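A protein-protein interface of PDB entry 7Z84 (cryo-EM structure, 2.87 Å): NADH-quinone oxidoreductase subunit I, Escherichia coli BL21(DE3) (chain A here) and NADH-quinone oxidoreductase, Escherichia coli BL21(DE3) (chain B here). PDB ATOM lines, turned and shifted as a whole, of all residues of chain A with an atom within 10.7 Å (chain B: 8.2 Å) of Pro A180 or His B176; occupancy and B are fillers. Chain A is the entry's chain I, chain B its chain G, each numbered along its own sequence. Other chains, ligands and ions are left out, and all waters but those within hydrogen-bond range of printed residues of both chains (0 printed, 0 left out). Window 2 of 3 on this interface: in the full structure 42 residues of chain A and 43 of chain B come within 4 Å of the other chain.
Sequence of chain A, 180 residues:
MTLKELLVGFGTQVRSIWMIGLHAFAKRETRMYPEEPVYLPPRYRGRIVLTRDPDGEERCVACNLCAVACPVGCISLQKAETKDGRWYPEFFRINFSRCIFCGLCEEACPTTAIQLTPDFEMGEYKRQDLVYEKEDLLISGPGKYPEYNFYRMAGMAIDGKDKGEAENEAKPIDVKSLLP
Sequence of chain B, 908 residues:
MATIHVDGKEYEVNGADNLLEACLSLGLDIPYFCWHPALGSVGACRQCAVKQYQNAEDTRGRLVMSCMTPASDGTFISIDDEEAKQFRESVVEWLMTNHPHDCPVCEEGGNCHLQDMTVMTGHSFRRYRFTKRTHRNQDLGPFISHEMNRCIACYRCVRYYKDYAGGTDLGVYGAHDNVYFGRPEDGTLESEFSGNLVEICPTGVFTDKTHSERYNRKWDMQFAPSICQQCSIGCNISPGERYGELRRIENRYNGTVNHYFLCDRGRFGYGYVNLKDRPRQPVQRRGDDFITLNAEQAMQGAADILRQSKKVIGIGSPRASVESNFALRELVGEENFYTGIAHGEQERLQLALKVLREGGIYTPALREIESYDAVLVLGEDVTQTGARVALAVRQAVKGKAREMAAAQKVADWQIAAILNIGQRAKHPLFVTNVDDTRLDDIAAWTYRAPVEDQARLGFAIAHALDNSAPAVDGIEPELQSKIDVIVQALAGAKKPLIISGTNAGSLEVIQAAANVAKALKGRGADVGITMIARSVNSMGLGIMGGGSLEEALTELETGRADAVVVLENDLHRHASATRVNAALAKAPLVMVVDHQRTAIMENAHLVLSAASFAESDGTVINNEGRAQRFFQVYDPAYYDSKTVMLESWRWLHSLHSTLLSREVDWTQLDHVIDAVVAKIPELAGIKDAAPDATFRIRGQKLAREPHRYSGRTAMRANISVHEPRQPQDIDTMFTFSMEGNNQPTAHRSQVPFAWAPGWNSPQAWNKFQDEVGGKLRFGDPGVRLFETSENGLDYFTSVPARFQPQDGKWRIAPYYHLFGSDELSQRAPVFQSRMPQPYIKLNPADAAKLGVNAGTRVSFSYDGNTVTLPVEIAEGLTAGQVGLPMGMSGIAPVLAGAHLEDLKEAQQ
Of the 8 printed residues of chain A, 4 touch a printed residue of chain B. Printed residues of chain A that touch a printed residue of chain B: Ile A173, Asp A174, Val A175 and Pro A180. Hydrophobic or aromatic side chains of chain A that line the printed part of chain B: Ile A173 and Val A175. Of the 9 printed residues of chain B, 4 touch a printed residue of chain A. Hydrophobic or aromatic side chains of chain B that line the printed part of chain A: His B176.
Printed residues of chain B within 4 Å of Ile A173: Asn B178. Printed residues of chain B within 4 Å of Asp A174: Asn B178 (3.7 Å). Leu A179 touches none of the printed residues of chain B. Of chain B, only His B176 (3.6 Å) comes within 4 Å of Pro A180. Tyr B155 touches none of the printed residues of chain A. Of the printed residues of chain A, Gly B174 touches Val A175 (3.7 Å). No residue of chain A comes within 4 Å of Asp B177. Asn B178 touches just these residues of chain A: Ile A173 (2.5 Å), Asp A174 (3.7 Å) and Val A175 (3.3 Å). The nearest residue of chain B that does not touch Pro A180 is Ala B175 (5.9 Å). The nearest residue of chain A that does not touch His B176 is Leu A179 (5.5 Å). The nearest printed residue of chain A that does not touch Tyr B173 is Lys A176 (7.2 Å).
Among the printed residues, merely in contact across the chains: Asp A174 with Asn B178, Val A175 with Tyr B173, Val A175 with Gly B174, Val A175 with Asn B178 and Pro A180 with His B176.
The side-chain amide nitrogen (ND2) of Asn B178 lies within hydrogen-bond range of the backbone carbonyl oxygen (O) of Ile A173 (2.5 Å).
ND1 of His B176 sits at hydrogen-bond distance from OD2 of Asp B177 (2.6 Å). The side-chain amino group (NZ) of Lys A176 lies within salt-bridge range of the side-chain carboxylate (OD1) of Asp A174. The backbone carbonyl oxygen (O) of Asp A174 is in hydrogen-bond range of the side-chain hydroxyl (OG) of Ser A177 (3.2 Å).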
ATOM      1  N   ILE A 173       8.354 -26.756   2.856  1.00  0.00           N
ATOM      2  CA  ILE A 173       9.360 -25.729   3.090  1.00  0.00           C
ATOM      3  C   ILE A 173       9.253 -24.708   1.969  1.00  0.00           C
ATOM      4  O   ILE A 173       9.339 -25.060   0.786  1.00  0.00           O
ATOM      5  CB  ILE A 173      10.771 -26.330   3.159  1.00  0.00           C
ATOM      6  CG1 ILE A 173      10.849 -27.384   4.263  1.00  0.00           C
ATOM      7  CG2 ILE A 173      11.804 -25.241   3.381  1.00  0.00           C
ATOM      8  CD1 ILE A 173      12.015 -28.329   4.118  1.00  0.00           C
ATOM      9  N   ASP A 174       9.055 -23.447   2.337  1.00  0.00           N
ATOM     10  CA  ASP A 174       8.972 -22.383   1.349  1.00  0.00           C
ATOM     11  C   ASP A 174      10.342 -22.111   0.738  1.00  0.00           C
ATOM     12  O   ASP A 174      11.381 -22.297   1.374  1.00  0.00           O
ATOM     13  CB  ASP A 174       8.421 -21.109   1.984  1.00  0.00           C
ATOM     14  CG  ASP A 174       7.535 -20.324   1.040  1.00  0.00           C
ATOM     15  OD1 ASP A 174       7.661 -19.084   0.999  1.00  0.00           O
ATOM     16  OD2 ASP A 174       6.712 -20.949   0.340  1.00  0.00           O
ATOM     17  N   VAL A 175      10.332 -21.667  -0.522  1.00  0.00           N
ATOM     18  CA  VAL A 175      11.575 -21.291  -1.184  1.00  0.00           C
ATOM     19  C   VAL A 175      12.114 -19.973  -0.649  1.00  0.00           C
ATOM     20  O   VAL A 175      13.284 -19.646  -0.877  1.00  0.00           O
ATOM     21  CB  VAL A 175      11.369 -21.218  -2.708  1.00  0.00           C
ATOM     22  CG1 VAL A 175      11.170 -22.609  -3.278  1.00  0.00           C
ATOM     23  CG2 VAL A 175      10.185 -20.329  -3.042  1.00  0.00           C
ATOM     24  N   LYS A 176      11.289 -19.210   0.063  1.00  0.00           N
ATOM     25  CA  LYS A 176      11.687 -17.951   0.673  1.00  0.00           C
ATOM     26  C   LYS A 176      12.228 -18.126   2.086  1.00  0.00           C
ATOM     27  O   LYS A 176      12.490 -17.126   2.762  1.00  0.00           O
ATOM     28  CB  LYS A 176      10.502 -16.983   0.689  1.00  0.00           C
ATOM     29  CG  LYS A 176       9.704 -16.959  -0.602  1.00  0.00           C
ATOM     30  CD  LYS A 176       9.234 -15.557  -0.936  1.00  0.00           C
ATOM     31  CE  LYS A 176       8.011 -15.181  -0.120  1.00  0.00           C
ATOM     32  NZ  LYS A 176       6.985 -16.258  -0.134  1.00  0.00           N
ATOM     33  N   SER A 177      12.384 -19.363   2.548  1.00  0.00           N
ATOM     34  CA  SER A 177      12.877 -19.614   3.895  1.00  0.00           C
ATOM     35  C   SER A 177      14.343 -19.214   4.022  1.00  0.00           C
ATOM     36  O   SER A 177      15.115 -19.276   3.063  1.00  0.00           O
ATOM     37  CB  SER A 177      12.705 -21.087   4.262  1.00  0.00           C
ATOM     38  OG  SER A 177      13.625 -21.897   3.552  1.00  0.00           O
ATOM     39  N   LEU A 178      14.720 -18.798   5.232  1.00  0.00           N
ATOM     40  CA  LEU A 178      16.069 -18.310   5.483  1.00  0.00           C
ATOM     41  C   LEU A 178      17.091 -19.427   5.629  1.00  0.00           C
ATOM     42  O   LEU A 178      18.293 -19.165   5.513  1.00  0.00           O
ATOM     43  CB  LEU A 178      16.083 -17.444   6.742  1.00  0.00           C
ATOM     44  CG  LEU A 178      14.956 -16.419   6.864  1.00  0.00           C
ATOM     45  CD1 LEU A 178      14.906 -15.858   8.272  1.00  0.00           C
ATOM     46  CD2 LEU A 178      15.140 -15.309   5.846  1.00  0.00           C
ATOM     47  N   LEU A 179      16.649 -20.653   5.889  1.00  0.00           N
ATOM     48  CA  LEU A 179      17.581 -21.753   6.080  1.00  0.00           C
ATOM     49  C   LEU A 179      18.200 -22.156   4.743  1.00  0.00           C
ATOM     50  O   LEU A 179      17.515 -22.157   3.717  1.00  0.00           O
ATOM     51  CB  LEU A 179      16.873 -22.949   6.714  1.00  0.00           C
ATOM     52  CG  LEU A 179      16.440 -22.777   8.170  1.00  0.00           C
ATOM     53  CD1 LEU A 179      15.446 -23.855   8.568  1.00  0.00           C
ATOM     54  CD2 LEU A 179      17.644 -22.792   9.092  1.00  0.00           C
ATOM     55  N   PRO A 180      19.498 -22.498   4.719  1.00  0.00           N
ATOM     56  CA  PRO A 180      20.179 -22.916   3.488  1.00  0.00           C
ATOM     57  C   PRO A 180      19.665 -24.247   2.941  1.00  0.00           C
ATOM     58  O   PRO A 180      19.012 -24.992   3.671  1.00  0.00           O
ATOM     59  CB  PRO A 180      21.646 -23.042   3.920  1.00  0.00           C
ATOM     60  CG  PRO A 180      21.753 -22.259   5.183  1.00  0.00           C
ATOM     61  CD  PRO A 180      20.430 -22.415   5.856  1.00  0.00           C
ATOM     62  N   ALA B 153      11.460 -32.272 -11.130  1.00  0.00           N
ATOM     63  CA  ALA B 153      12.495 -31.264 -11.388  1.00  0.00           C
ATOM     64  C   ALA B 153      13.240 -31.527 -12.693  1.00  0.00           C
ATOM     65  O   ALA B 153      14.470 -31.540 -12.744  1.00  0.00           O
ATOM     66  CB  ALA B 153      13.466 -31.154 -10.211  1.00  0.00           C
ATOM     67  N   TYR B 155      12.742 -29.652 -15.485  1.00  0.00           N
ATOM     68  CA  TYR B 155      12.936 -28.342 -16.113  1.00  0.00           C
ATOM     69  C   TYR B 155      12.346 -28.255 -17.517  1.00  0.00           C
ATOM     70  O   TYR B 155      12.753 -27.399 -18.302  1.00  0.00           O
ATOM     71  CB  TYR B 155      14.419 -27.940 -16.146  1.00  0.00           C
ATOM     72  CG  TYR B 155      15.034 -27.724 -14.784  1.00  0.00           C
ATOM     73  CD1 TYR B 155      15.536 -28.789 -14.050  1.00  0.00           C
ATOM     74  CD2 TYR B 155      15.118 -26.453 -14.234  1.00  0.00           C
ATOM     75  CE1 TYR B 155      16.100 -28.597 -12.806  1.00  0.00           C
ATOM     76  CE2 TYR B 155      15.678 -26.251 -12.989  1.00  0.00           C
ATOM     77  CZ  TYR B 155      16.167 -27.327 -12.280  1.00  0.00           C
ATOM     78  OH  TYR B 155      16.729 -27.132 -11.042  1.00  0.00           O
ATOM     79  N   TYR B 173      12.368 -21.641  -8.874  1.00  0.00           N
ATOM     80  CA  TYR B 173      12.755 -20.924  -7.671  1.00  0.00           C
ATOM     81  C   TYR B 173      13.298 -21.914  -6.658  1.00  0.00           C
ATOM     82  O   TYR B 173      12.966 -23.100  -6.689  1.00  0.00           O
ATOM     83  CB  TYR B 173      11.567 -20.171  -7.066  1.00  0.00           C
ATOM     84  CG  TYR B 173      10.669 -19.582  -8.114  1.00  0.00           C
ATOM     85  CD1 TYR B 173      11.032 -18.437  -8.805  1.00  0.00           C
ATOM     86  CD2 TYR B 173       9.469 -20.191  -8.435  1.00  0.00           C
ATOM     87  CE1 TYR B 173      10.220 -17.908  -9.775  1.00  0.00           C
ATOM     88  CE2 TYR B 173       8.652 -19.671  -9.397  1.00  0.00           C
ATOM     89  CZ  TYR B 173       9.030 -18.529 -10.067  1.00  0.00           C
ATOM     90  OH  TYR B 173       8.213 -18.010 -11.037  1.00  0.00           O
ATOM     91  N   GLY B 174      14.137 -21.421  -5.760  1.00  0.00           N
ATOM     92  CA  GLY B 174      14.594 -22.257  -4.676  1.00  0.00           C
ATOM     93  C   GLY B 174      15.937 -22.916  -4.892  1.00  0.00           C
ATOM     94  O   GLY B 174      16.807 -22.383  -5.585  1.00  0.00           O
ATOM     95  N   ALA B 175      16.100 -24.098  -4.308  1.00  0.00           N
ATOM     96  CA  ALA B 175      17.419 -24.656  -4.058  1.00  0.00           C
ATOM     97  C   ALA B 175      17.407 -26.175  -4.134  1.00  0.00           C
ATOM     98  O   ALA B 175      16.508 -26.768  -4.736  1.00  0.00           O
ATOM     99  CB  ALA B 175      17.943 -24.194  -2.698  1.00  0.00           C
ATOM    100  N   HIS B 176      18.390 -26.785  -3.476  1.00  0.00           N
ATOM    101  CA  HIS B 176      18.894 -28.148  -3.619  1.00  0.00           C
ATOM    102  C   HIS B 176      17.875 -29.238  -3.936  1.00  0.00           C
ATOM    103  O   HIS B 176      17.984 -29.905  -4.966  1.00  0.00           O
ATOM    104  CB  HIS B 176      19.581 -28.503  -2.307  1.00  0.00           C
ATOM    105  CG  HIS B 176      18.961 -27.837  -1.116  1.00  0.00           C
ATOM    106  ND1 HIS B 176      17.881 -28.369  -0.445  1.00  0.00           N
ATOM    107  CD2 HIS B 176      19.245 -26.667  -0.497  1.00  0.00           C
ATOM    108  CE1 HIS B 176      17.539 -27.565   0.544  1.00  0.00           C
ATOM    109  NE2 HIS B 176      18.351 -26.524   0.535  1.00  0.00           N
ATOM    110  N   ASP B 177      16.892 -29.435  -3.068  1.00  0.00           N
ATOM    111  CA  ASP B 177      15.807 -30.363  -3.335  1.00  0.00           C
ATOM    112  C   ASP B 177      14.447 -29.705  -3.188  1.00  0.00           C
ATOM    113  O   ASP B 177      13.423 -30.370  -3.381  1.00  0.00           O
ATOM    114  CB  ASP B 177      15.908 -31.595  -2.420  1.00  0.00           C
ATOM    115  CG  ASP B 177      15.775 -31.253  -0.947  1.00  0.00           C
ATOM    116  OD1 ASP B 177      15.495 -32.174  -0.151  1.00  0.00           O
ATOM    117  OD2 ASP B 177      15.975 -30.078  -0.574  1.00  0.00           O
ATOM    118  N   ASN B 178      14.414 -28.413  -2.864  1.00  0.00           N
ATOM    119  CA  ASN B 178      13.186 -27.641  -2.747  1.00  0.00           C
ATOM    120  C   ASN B 178      12.940 -26.770  -3.972  1.00  0.00           C
ATOM    121  O   ASN B 178      12.468 -25.636  -3.838  1.00  0.00           O
ATOM    122  CB  ASN B 178      13.225 -26.782  -1.485  1.00  0.00           C
ATOM    123  CG  ASN B 178      11.913 -26.792  -0.733  1.00  0.00           C
ATOM    124  OD1 ASN B 178      11.224 -27.809  -0.677  1.00  0.00           O
ATOM    125  ND2 ASN B 178      11.557 -25.654  -0.154  1.00  0.00           N
ATOM    126  N   VAL B 179      13.272 -27.268  -5.165  1.00  0.00           N
ATOM    127  CA  VAL B 179      13.015 -26.518  -6.390  1.00  0.00           C
ATOM    128  C   VAL B 179      11.517 -26.436  -6.635  1.00  0.00           C
ATOM    129  O   VAL B 179      10.799 -27.442  -6.572  1.00  0.00           O
ATOM    130  CB  VAL B 179      13.740 -27.152  -7.585  1.00  0.00           C
ATOM    131  CG1 VAL B 179      15.174 -26.687  -7.646  1.00  0.00           C
ATOM    132  CG2 VAL B 179      13.697 -28.663  -7.485  1.00  0.00           C
